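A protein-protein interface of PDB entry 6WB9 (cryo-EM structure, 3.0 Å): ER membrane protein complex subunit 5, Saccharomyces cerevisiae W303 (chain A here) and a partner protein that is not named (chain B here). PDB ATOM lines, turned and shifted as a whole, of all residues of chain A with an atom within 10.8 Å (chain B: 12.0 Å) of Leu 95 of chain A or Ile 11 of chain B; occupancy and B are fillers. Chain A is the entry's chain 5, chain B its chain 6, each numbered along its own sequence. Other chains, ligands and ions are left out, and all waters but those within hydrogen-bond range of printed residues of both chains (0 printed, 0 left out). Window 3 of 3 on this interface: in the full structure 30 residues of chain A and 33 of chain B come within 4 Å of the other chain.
O of Lys 91 of chain A is in hydrogen-bond range of ND2 of Asn 20 of chain B (2.5 Å). ND2 of Asn 16 of chain B lies within hydrogen-bond range of O of Glu 92 of chain A (2.4 Å). OE2 of Glu 92 of chain A is in salt-bridge range of NZ of Lys 75 of chain B. The backbone carbonyl oxygen of Ile 93 of chain A lies within hydrogen-bond range of the backbone NH of Ala 13 of chain B (2.6 Å). The backbone carbonyl oxygen (O) of Lys 75 of chain B sits at hydrogen-bond distance from the backbone NH (N) of Ile 93 of chain A (3.0 Å). O of Ile 11 of chain B lies within hydrogen-bond range of N of Leu 95 of chain A, at 3.0 Å.
Among the printed residues, merely in contact across the chains: Ile 93 of chain A with Asn 12 of chain B, Ile 93 of chain A with Phe 76 of chain B, Ile 93 of chain A with Gln 78 of chain B, Lys 91 of chain A with Asn 16 of chain B, Ala 98 of chain A with Asn 16 of chain B, Ala 94 of chain A with Gln 10 of chain B, Ile 93 of chain A with Asn 20 of chain B, Lys 91 of chain A with Phe 76 of chain B, Ile 93 of chain A with Val 17 of chain B, Ala 98 of chain A with Ala 13 of chain B, Ala 94 of chain A with Ile 11 of chain B, Ile 93 of chain A with Tyr 77 of chain B, Leu 95 of chain A with Ala 13 of chain B, Glu 92 of chain A with Phe 76 of chain B and Ile 93 of chain A with Asn 16 of chain B.
Printed residues of chain B that touch a printed residue of chain A: Gln 10, Ile 11, Asn 12, Ala 13, Asn 16, Val 17, Asn 20, Lys 75, Phe 76, Tyr 77 and Gln 78. Hydrophobic or aromatic side chains of chain B that line the printed part of chain A: Ile 11, Ala 13, Val 17 and Phe 76. Hydrophobic or aromatic side chains of chain A that line the printed part of chain B: Ile 93, Ala 94, Leu 95 and Ala 98. Among the printed residues, 21 pairs touch across the chains. Among the printed residues, Asp or Glu carboxylates within 4 Å of a Lys or Arg side-chain nitrogen of the other chain: Glu 92 of chain A with Lys 75 of chain B.
The side-chain hydroxyl (OG1) of Thr 99 of chain A lies within hydrogen-bond range of the backbone carbonyl oxygen (O) of Leu 95 of chain A, 2.9 Å away. The side-chain amide oxygen (OE1) of Gln 10 of chain B lies close to the side-chain amide oxygen (OD1) of Asn 12 of chain B (2.9 Å). OE1 of Gln 78 of chain B lies within hydrogen-bond range of ND2 of Asn 12 of chain B (3.2 Å). ND2 of Asn 20 of chain B lies close to O of Asn 16 of chain B. The side-chain amide nitrogen (ND2) of Asn 20 of chain B is in hydrogen-bond range of the backbone carbonyl oxygen (O) of Phe 76 of chain B, 2.7 Å away. O of Asn 20 of chain B is in hydrogen-bond range of OH of Tyr 77 of chain B.
Of chain B, only Ile 11 (3.0 Å) and Ala 13 (3.9 Å) come within 4 Å of Leu 95 of chain A. Ile 11 of chain B touches two residues of chain A. Of the printed residues of chain B, Ala 98 of chain A touches Ala 13 (3.7 Å) and Asn 16 (3.5 Å). Of chain A, only Ala 94 (3.5 Å) comes within 4 Å of Gln 10 of chain B. Printed residues of chain A within 4 Å of Lys 75 of chain B: Glu 92 and Ile 93. Of the printed residues of chain B, Glu 92 of chain A touches Asn 16, Lys 75 and Phe 76. Printed residues of chain A within 4 Å of Tyr 77 of chain B: Ile 93 (3.9 Å). Printed residues of chain A within 4 Å of Val 17 of chain B: Ile 93 (3.7 Å). Asn 110 of chain A touches none of the printed residues of chain B.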
ATOM      1  N   GLN A  86      28.608 -23.728  17.555  1.00  0.00           N
ATOM      2  CA  GLN A  86      29.502 -22.964  18.413  1.00  0.00           C
ATOM      3  C   GLN A  86      30.034 -23.773  19.584  1.00  0.00           C
ATOM      4  O   GLN A  86      30.879 -23.269  20.330  1.00  0.00           O
ATOM      5  CB  GLN A  86      28.792 -21.723  18.950  1.00  0.00           C
ATOM      6  CG  GLN A  86      28.374 -20.732  17.896  1.00  0.00           C
ATOM      7  CD  GLN A  86      27.974 -19.406  18.492  1.00  0.00           C
ATOM      8  OE1 GLN A  86      26.832 -19.219  18.905  1.00  0.00           O
ATOM      9  NE2 GLN A  86      28.918 -18.478  18.552  1.00  0.00           N
ATOM     10  N   LYS A  91      22.120 -20.894  24.919  1.00  0.00           N
ATOM     11  CA  LYS A  91      22.209 -19.766  24.007  1.00  0.00           C
ATOM     12  C   LYS A  91      22.794 -18.577  24.752  1.00  0.00           C
ATOM     13  O   LYS A  91      22.396 -18.295  25.886  1.00  0.00           O
ATOM     14  CB  LYS A  91      20.833 -19.427  23.434  1.00  0.00           C
ATOM     15  CG  LYS A  91      20.008 -20.660  23.118  1.00  0.00           C
ATOM     16  CD  LYS A  91      19.096 -20.451  21.930  1.00  0.00           C
ATOM     17  CE  LYS A  91      17.974 -19.491  22.257  1.00  0.00           C
ATOM     18  NZ  LYS A  91      17.060 -19.292  21.098  1.00  0.00           N
ATOM     19  N   GLU A  92      23.749 -17.898  24.121  1.00  0.00           N
ATOM     20  CA  GLU A  92      24.438 -16.792  24.769  1.00  0.00           C
ATOM     21  C   GLU A  92      23.517 -15.589  24.892  1.00  0.00           C
ATOM     22  O   GLU A  92      22.791 -15.243  23.959  1.00  0.00           O
ATOM     23  CB  GLU A  92      25.690 -16.415  23.987  1.00  0.00           C
ATOM     24  CG  GLU A  92      26.550 -17.599  23.614  1.00  0.00           C
ATOM     25  CD  GLU A  92      28.015 -17.247  23.538  1.00  0.00           C
ATOM     26  OE1 GLU A  92      28.440 -16.328  24.265  1.00  0.00           O
ATOM     27  OE2 GLU A  92      28.743 -17.890  22.754  1.00  0.00           O
ATOM     28  N   ILE A  93      23.544 -14.953  26.058  1.00  0.00           N
ATOM     29  CA  ILE A  93      22.607 -13.871  26.316  1.00  0.00           C
ATOM     30  C   ILE A  93      23.119 -12.529  25.811  1.00  0.00           C
ATOM     31  O   ILE A  93      22.313 -11.661  25.466  1.00  0.00           O
ATOM     32  CB  ILE A  93      22.258 -13.806  27.811  1.00  0.00           C
ATOM     33  CG1 ILE A  93      23.507 -13.616  28.664  1.00  0.00           C
ATOM     34  CG2 ILE A  93      21.555 -15.066  28.225  1.00  0.00           C
ATOM     35  CD1 ILE A  93      23.217 -13.051  30.019  1.00  0.00           C
ATOM     36  N   ALA A  94      24.436 -12.339  25.747  1.00  0.00           N
ATOM     37  CA  ALA A  94      24.994 -11.067  25.311  1.00  0.00           C
ATOM     38  C   ALA A  94      24.770 -10.884  23.818  1.00  0.00           C
ATOM     39  O   ALA A  94      25.096 -11.768  23.023  1.00  0.00           O
ATOM     40  CB  ALA A  94      26.483 -11.001  25.634  1.00  0.00           C
ATOM     41  N   LEU A  95      24.222  -9.721  23.444  1.00  0.00           N
ATOM     42  CA  LEU A  95      23.806  -9.459  22.069  1.00  0.00           C
ATOM     43  C   LEU A  95      24.975  -9.426  21.090  1.00  0.00           C
ATOM     44  O   LEU A  95      24.762  -9.637  19.892  1.00  0.00           O
ATOM     45  CB  LEU A  95      23.029  -8.143  22.016  1.00  0.00           C
ATOM     46  CG  LEU A  95      22.185  -7.832  20.781  1.00  0.00           C
ATOM     47  CD1 LEU A  95      21.115  -8.884  20.569  1.00  0.00           C
ATOM     48  CD2 LEU A  95      21.570  -6.461  20.917  1.00  0.00           C
ATOM     49  N   ASN A  96      26.194  -9.168  21.572  1.00  0.00           N
ATOM     50  CA  ASN A  96      27.388  -9.374  20.757  1.00  0.00           C
ATOM     51  C   ASN A  96      27.503 -10.827  20.317  1.00  0.00           C
ATOM     52  O   ASN A  96      27.767 -11.118  19.146  1.00  0.00           O
ATOM     53  CB  ASN A  96      28.638  -8.974  21.542  1.00  0.00           C
ATOM     54  CG  ASN A  96      28.591  -7.550  22.030  1.00  0.00           C
ATOM     55  OD1 ASN A  96      29.099  -6.646  21.372  1.00  0.00           O
ATOM     56  ND2 ASN A  96      28.000  -7.341  23.200  1.00  0.00           N
ATOM     57  N   LYS A  97      27.290 -11.753  21.247  1.00  0.00           N
ATOM     58  CA  LYS A  97      27.433 -13.174  20.981  1.00  0.00           C
ATOM     59  C   LYS A  97      26.106 -13.877  20.729  1.00  0.00           C
ATOM     60  O   LYS A  97      26.114 -15.031  20.293  1.00  0.00           O
ATOM     61  CB  LYS A  97      28.156 -13.852  22.149  1.00  0.00           C
ATOM     62  CG  LYS A  97      29.660 -14.021  21.959  1.00  0.00           C
ATOM     63  CD  LYS A  97      30.419 -12.715  22.113  1.00  0.00           C
ATOM     64  CE  LYS A  97      30.311 -12.172  23.523  1.00  0.00           C
ATOM     65  NZ  LYS A  97      31.127 -10.940  23.703  1.00  0.00           N
ATOM     66  N   ALA A  98      24.975 -13.220  20.994  1.00  0.00           N
ATOM     67  CA  ALA A  98      23.686 -13.832  20.691  1.00  0.00           C
ATOM     68  C   ALA A  98      23.429 -13.850  19.196  1.00  0.00           C
ATOM     69  O   ALA A  98      22.854 -14.808  18.667  1.00  0.00           O
ATOM     70  CB  ALA A  98      22.562 -13.090  21.406  1.00  0.00           C
ATOM     71  N   THR A  99      23.847 -12.801  18.501  1.00  0.00           N
ATOM     72  CA  THR A  99      23.674 -12.684  17.063  1.00  0.00           C
ATOM     73  C   THR A  99      24.786 -13.363  16.281  1.00  0.00           C
ATOM     74  O   THR A  99      24.794 -13.285  15.047  1.00  0.00           O
ATOM     75  CB  THR A  99      23.590 -11.213  16.674  1.00  0.00           C
ATOM     76  OG1 THR A  99      24.761 -10.543  17.143  1.00  0.00           O
ATOM     77  CG2 THR A  99      22.375 -10.573  17.309  1.00  0.00           C
ATOM     78  N   ASN A 100      25.720 -14.029  16.964  1.00  0.00           N
ATOM     79  CA  ASN A 100      26.707 -14.844  16.268  1.00  0.00           C
ATOM     80  C   ASN A 100      26.057 -16.034  15.584  1.00  0.00           C
ATOM     81  O   ASN A 100      26.534 -16.472  14.538  1.00  0.00           O
ATOM     82  CB  ASN A 100      27.785 -15.321  17.238  1.00  0.00           C
ATOM     83  CG  ASN A 100      28.805 -14.250  17.541  1.00  0.00           C
ATOM     84  OD1 ASN A 100      28.634 -13.094  17.163  1.00  0.00           O
ATOM     85  ND2 ASN A 100      29.873 -14.628  18.228  1.00  0.00           N
ATOM     86  N   VAL A 101      24.970 -16.557  16.156  1.00  0.00           N
ATOM     87  CA  VAL A 101      24.189 -17.601  15.497  1.00  0.00           C
ATOM     88  C   VAL A 101      23.592 -17.078  14.199  1.00  0.00           C
ATOM     89  O   VAL A 101      23.632 -17.750  13.163  1.00  0.00           O
ATOM     90  CB  VAL A 101      23.099 -18.117  16.453  1.00  0.00           C
ATOM     91  CG1 VAL A 101      22.159 -19.071  15.746  1.00  0.00           C
ATOM     92  CG2 VAL A 101      23.731 -18.784  17.655  1.00  0.00           C
ATOM     93  N   ASP A 102      23.075 -15.850  14.226  1.00  0.00           N
ATOM     94  CA  ASP A 102      22.439 -15.280  13.047  1.00  0.00           C
ATOM     95  C   ASP A 102      23.456 -14.876  11.989  1.00  0.00           C
ATOM     96  O   ASP A 102      23.142 -14.891  10.796  1.00  0.00           O
ATOM     97  CB  ASP A 102      21.588 -14.086  13.463  1.00  0.00           C
ATOM     98  CG  ASP A 102      20.654 -14.418  14.608  1.00  0.00           C
ATOM     99  OD1 ASP A 102      19.887 -15.396  14.484  1.00  0.00           O
ATOM    100  OD2 ASP A 102      20.698 -13.717  15.640  1.00  0.00           O
ATOM    101  N   ASN A 103      24.671 -14.521  12.399  1.00  0.00           N
ATOM    102  CA  ASN A 103      25.709 -14.164  11.441  1.00  0.00           C
ATOM    103  C   ASN A 103      26.456 -15.372  10.894  1.00  0.00           C
ATOM    104  O   ASN A 103      26.979 -15.309   9.776  1.00  0.00           O
ATOM    105  CB  ASN A 103      26.704 -13.196  12.080  1.00  0.00           C
ATOM    106  CG  ASN A 103      26.067 -11.885  12.469  1.00  0.00           C
ATOM    107  OD1 ASN A 103      25.284 -11.314  11.714  1.00  0.00           O
ATOM    108  ND2 ASN A 103      26.390 -11.404  13.658  1.00  0.00           N
ATOM    109  N   ASN A 108      19.199 -12.773   9.273  1.00  0.00           N
ATOM    110  CA  ASN A 108      19.098 -11.428   9.811  1.00  0.00           C
ATOM    111  C   ASN A 108      17.877 -11.394  10.717  1.00  0.00           C
ATOM    112  O   ASN A 108      16.757 -11.563  10.224  1.00  0.00           O
ATOM    113  CB  ASN A 108      18.980 -10.403   8.684  1.00  0.00           C
ATOM    114  CG  ASN A 108      19.496  -9.035   9.079  1.00  0.00           C
ATOM    115  OD1 ASN A 108      19.466  -8.654  10.248  1.00  0.00           O
ATOM    116  ND2 ASN A 108      19.974  -8.286   8.095  1.00  0.00           N
ATOM    117  N   PRO A 109      18.053 -11.194  12.030  1.00  0.00           N
ATOM    118  CA  PRO A 109      16.918 -11.311  12.965  1.00  0.00           C
ATOM    119  C   PRO A 109      15.822 -10.288  12.741  1.00  0.00           C
ATOM    120  O   PRO A 109      14.645 -10.595  12.962  1.00  0.00           O
ATOM    121  CB  PRO A 109      17.574 -11.120  14.340  1.00  0.00           C
ATOM    122  CG  PRO A 109      19.022 -11.321  14.119  1.00  0.00           C
ATOM    123  CD  PRO A 109      19.310 -10.896  12.727  1.00  0.00           C
ATOM    124  N   ASN A 110      16.172  -9.083  12.307  1.00  0.00           N
ATOM    125  CA  ASN A 110      15.181  -8.132  11.816  1.00  0.00           C
ATOM    126  C   ASN A 110      15.024  -8.243  10.306  1.00  0.00           C
ATOM    127  O   ASN A 110      15.053  -7.253   9.586  1.00  0.00           O
ATOM    128  CB  ASN A 110      15.575  -6.719  12.225  1.00  0.00           C
ATOM    129  CG  ASN A 110      15.690  -6.562  13.722  1.00  0.00           C
ATOM    130  OD1 ASN A 110      16.747  -6.798  14.304  1.00  0.00           O
ATOM    131  ND2 ASN A 110      14.597  -6.165  14.359  1.00  0.00           N
ATOM    132  N   GLN B  10      25.851  -4.225  29.903  1.00  0.00           N
ATOM    133  CA  GLN B  10      25.761  -5.255  28.877  1.00  0.00           C
ATOM    134  C   GLN B  10      24.351  -5.338  28.310  1.00  0.00           C
ATOM    135  O   GLN B  10      23.379  -5.433  29.056  1.00  0.00           O
ATOM    136  CB  GLN B  10      26.177  -6.615  29.439  1.00  0.00           C
ATOM    137  CG  GLN B  10      26.224  -7.724  28.403  1.00  0.00           C
ATOM    138  CD  GLN B  10      26.473  -9.085  29.018  1.00  0.00           C
ATOM    139  OE1 GLN B  10      25.675  -9.576  29.816  1.00  0.00           O
ATOM    140  NE2 GLN B  10      27.588  -9.704  28.652  1.00  0.00           N
ATOM    141  N   ILE B  11      24.249  -5.297  26.986  1.00  0.00           N
ATOM    142  CA  ILE B  11      22.970  -5.412  26.298  1.00  0.00           C
ATOM    143  C   ILE B  11      22.681  -6.889  26.079  1.00  0.00           C
ATOM    144  O   ILE B  11      23.420  -7.574  25.363  1.00  0.00           O
ATOM    145  CB  ILE B  11      22.984  -4.653  24.965  1.00  0.00           C
ATOM    146  CG1 ILE B  11      23.399  -3.201  25.188  1.00  0.00           C
ATOM    147  CG2 ILE B  11      21.623  -4.726  24.305  1.00  0.00           C
ATOM    148  CD1 ILE B  11      23.636  -2.438  23.912  1.00  0.00           C
ATOM    149  N   ASN B  12      21.611  -7.381  26.692  1.00  0.00           N
ATOM    150  CA  ASN B  12      21.246  -8.783  26.606  1.00  0.00           C
ATOM    151  C   ASN B  12      20.167  -9.002  25.555  1.00  0.00           C
ATOM    152  O   ASN B  12      19.379  -8.106  25.246  1.00  0.00           O
ATOM    153  CB  ASN B  12      20.755  -9.307  27.955  1.00  0.00           C
ATOM    154  CG  ASN B  12      21.869  -9.459  28.960  1.00  0.00           C
ATOM    155  OD1 ASN B  12      22.999  -9.786  28.606  1.00  0.00           O
ATOM    156  ND2 ASN B  12      21.559  -9.220  30.226  1.00  0.00           N
ATOM    157  N   ALA B  13      20.144 -10.212  25.004  1.00  0.00           N
ATOM    158  CA  ALA B  13      19.064 -10.669  24.140  1.00  0.00           C
ATOM    159  C   ALA B  13      18.095 -11.450  25.013  1.00  0.00           C
ATOM    160  O   ALA B  13      18.415 -12.553  25.463  1.00  0.00           O
ATOM    161  CB  ALA B  13      19.595 -11.527  22.998  1.00  0.00           C
ATOM    162  N   THR B  14      16.910 -10.877  25.248  1.00  0.00           N
ATOM    163  CA  THR B  14      16.000 -11.389  26.266  1.00  0.00           C
ATOM    164  C   THR B  14      15.400 -12.741  25.907  1.00  0.00           C
ATOM    165  O   THR B  14      15.002 -13.483  26.813  1.00  0.00           O
ATOM    166  CB  THR B  14      14.877 -10.386  26.520  1.00  0.00           C
ATOM    167  OG1 THR B  14      14.138 -10.178  25.312  1.00  0.00           O
ATOM    168  CG2 THR B  14      15.452  -9.061  26.989  1.00  0.00           C
ATOM    169  N   ALA B  15      15.334 -13.080  24.617  1.00  0.00           N
ATOM    170  CA  ALA B  15      14.858 -14.400  24.221  1.00  0.00           C
ATOM    171  C   ALA B  15      15.824 -15.485  24.672  1.00  0.00           C
ATOM    172  O   ALA B  15      15.400 -16.549  25.139  1.00  0.00           O
ATOM    173  CB  ALA B  15      14.655 -14.453  22.709  1.00  0.00           C
ATOM    174  N   ASN B  16      17.127 -15.213  24.584  1.00  0.00           N
ATOM    175  CA  ASN B  16      18.121 -16.162  25.069  1.00  0.00           C
ATOM    176  C   ASN B  16      18.111 -16.266  26.588  1.00  0.00           C
ATOM    177  O   ASN B  16      18.326 -17.357  27.124  1.00  0.00           O
ATOM    178  CB  ASN B  16      19.505 -15.767  24.568  1.00  0.00           C
ATOM    179  CG  ASN B  16      19.651 -15.945  23.078  1.00  0.00           C
ATOM    180  OD1 ASN B  16      18.669 -16.145  22.371  1.00  0.00           O
ATOM    181  ND2 ASN B  16      20.879 -15.878  22.591  1.00  0.00           N
ATOM    182  N   VAL B  17      17.837 -15.158  27.287  1.00  0.00           N
ATOM    183  CA  VAL B  17      17.719 -15.183  28.746  1.00  0.00           C
ATOM    184  C   VAL B  17      16.540 -16.049  29.170  1.00  0.00           C
ATOM    185  O   VAL B  17      16.656 -16.890  30.071  1.00  0.00           O
ATOM    186  CB  VAL B  17      17.577 -13.753  29.300  1.00  0.00           C
ATOM    187  CG1 VAL B  17      17.615 -13.764  30.814  1.00  0.00           C
ATOM    188  CG2 VAL B  17      18.653 -12.849  28.754  1.00  0.00           C
ATOM    189  N   VAL B  18      15.395 -15.865  28.505  1.00  0.00           N
ATOM    190  CA  VAL B  18      14.192 -16.630  28.820  1.00  0.00           C
ATOM    191  C   VAL B  18      14.384 -18.108  28.490  1.00  0.00           C
ATOM    192  O   VAL B  18      13.981 -18.983  29.265  1.00  0.00           O
ATOM    193  CB  VAL B  18      12.984 -16.014  28.087  1.00  0.00           C
ATOM    194  CG1 VAL B  18      11.782 -16.940  28.088  1.00  0.00           C
ATOM    195  CG2 VAL B  18      12.608 -14.696  28.732  1.00  0.00           C
ATOM    196  N   ASN B  20      17.319 -19.814  28.361  1.00  0.00           N
ATOM    197  CA  ASN B  20      18.259 -20.406  29.307  1.00  0.00           C
ATOM    198  C   ASN B  20      17.618 -20.615  30.671  1.00  0.00           C
ATOM    199  O   ASN B  20      17.858 -21.640  31.323  1.00  0.00           O
ATOM    200  CB  ASN B  20      19.501 -19.530  29.428  1.00  0.00           C
ATOM    201  CG  ASN B  20      20.315 -19.506  28.166  1.00  0.00           C
ATOM    202  OD1 ASN B  20      20.173 -20.373  27.312  1.00  0.00           O
ATOM    203  ND2 ASN B  20      21.171 -18.507  28.036  1.00  0.00           N
ATOM    204  N   GLY B  74      28.177 -17.057  33.183  1.00  0.00           N
ATOM    205  CA  GLY B  74      27.936 -15.638  33.009  1.00  0.00           C
ATOM    206  C   GLY B  74      27.556 -15.237  31.604  1.00  0.00           C
ATOM    207  O   GLY B  74      26.913 -14.200  31.422  1.00  0.00           O
ATOM    208  N   LYS B  75      27.945 -16.027  30.607  1.00  0.00           N
ATOM    209  CA  LYS B  75      27.524 -15.786  29.237  1.00  0.00           C
ATOM    210  C   LYS B  75      26.168 -16.397  28.928  1.00  0.00           C
ATOM    211  O   LYS B  75      25.618 -16.138  27.854  1.00  0.00           O
ATOM    212  CB  LYS B  75      28.567 -16.330  28.258  1.00  0.00           C
ATOM    213  CG  LYS B  75      29.035 -17.724  28.573  1.00  0.00           C
ATOM    214  CD  LYS B  75      30.257 -18.095  27.759  1.00  0.00           C
ATOM    215  CE  LYS B  75      29.896 -18.453  26.335  1.00  0.00           C
ATOM    216  NZ  LYS B  75      31.080 -18.926  25.571  1.00  0.00           N
ATOM    217  N   PHE B  76      25.621 -17.191  29.844  1.00  0.00           N
ATOM    218  CA  PHE B  76      24.326 -17.822  29.675  1.00  0.00           C
ATOM    219  C   PHE B  76      23.284 -17.347  30.671  1.00  0.00           C
ATOM    220  O   PHE B  76      22.089 -17.494  30.400  1.00  0.00           O
ATOM    221  CB  PHE B  76      24.462 -19.346  29.794  1.00  0.00           C
ATOM    222  CG  PHE B  76      25.444 -19.940  28.836  1.00  0.00           C
ATOM    223  CD1 PHE B  76      25.423 -19.588  27.501  1.00  0.00           C
ATOM    224  CD2 PHE B  76      26.396 -20.843  29.270  1.00  0.00           C
ATOM    225  CE1 PHE B  76      26.325 -20.134  26.613  1.00  0.00           C
ATOM    226  CE2 PHE B  76      27.301 -21.391  28.384  1.00  0.00           C
ATOM    227  CZ  PHE B  76      27.263 -21.035  27.056  1.00  0.00           C
ATOM    228  N   TYR B  77      23.696 -16.799  31.811  1.00  0.00           N
ATOM    229  CA  TYR B  77      22.780 -16.276  32.818  1.00  0.00           C
ATOM    230  C   TYR B  77      23.364 -14.983  33.354  1.00  0.00           C
ATOM    231  O   TYR B  77      24.502 -14.971  33.828  1.00  0.00           O
ATOM    232  CB  TYR B  77      22.569 -17.275  33.963  1.00  0.00           C
ATOM    233  CG  TYR B  77      21.994 -18.593  33.518  1.00  0.00           C
ATOM    234  CD1 TYR B  77      20.624 -18.769  33.406  1.00  0.00           C
ATOM    235  CD2 TYR B  77      22.820 -19.655  33.194  1.00  0.00           C
ATOM    236  CE1 TYR B  77      20.099 -19.964  32.989  1.00  0.00           C
ATOM    237  CE2 TYR B  77      22.301 -20.849  32.773  1.00  0.00           C
ATOM    238  CZ  TYR B  77      20.943 -20.997  32.671  1.00  0.00           C
ATOM    239  OH  TYR B  77      20.428 -22.195  32.249  1.00  0.00           O
ATOM    240  N   GLN B  78      22.606 -13.897  33.275  1.00  0.00           N
ATOM    241  CA  GLN B  78      23.006 -12.680  33.962  1.00  0.00           C
ATOM    242  C   GLN B  78      22.731 -12.854  35.448  1.00  0.00           C
ATOM    243  O   GLN B  78      21.634 -13.271  35.832  1.00  0.00           O
ATOM    244  CB  GLN B  78      22.267 -11.461  33.410  1.00  0.00           C
ATOM    245  CG  GLN B  78      20.796 -11.672  33.121  1.00  0.00           C
ATOM    246  CD  GLN B  78      20.053 -10.364  32.976  1.00  0.00           C
ATOM    247  OE1 GLN B  78      20.584  -9.302  33.297  1.00  0.00           O
ATOM    248  NE2 GLN B  78      18.820 -10.430  32.492  1.00  0.00           N
ATOM    249  N   SER B  79      23.733 -12.525  36.277  1.00  0.00           N
ATOM    250  CA  SER B  79      23.809 -12.856  37.700  1.00  0.00           C
ATOM    251  C   SER B  79      23.595 -14.355  37.886  1.00  0.00           C
ATOM    252  O   SER B  79      22.497 -14.776  38.267  1.00  0.00           O
ATOM    253  CB  SER B  79      22.805 -12.050  38.530  1.00  0.00           C
ATOM    254  OG  SER B  79      21.475 -12.444  38.254  1.00  0.00           O
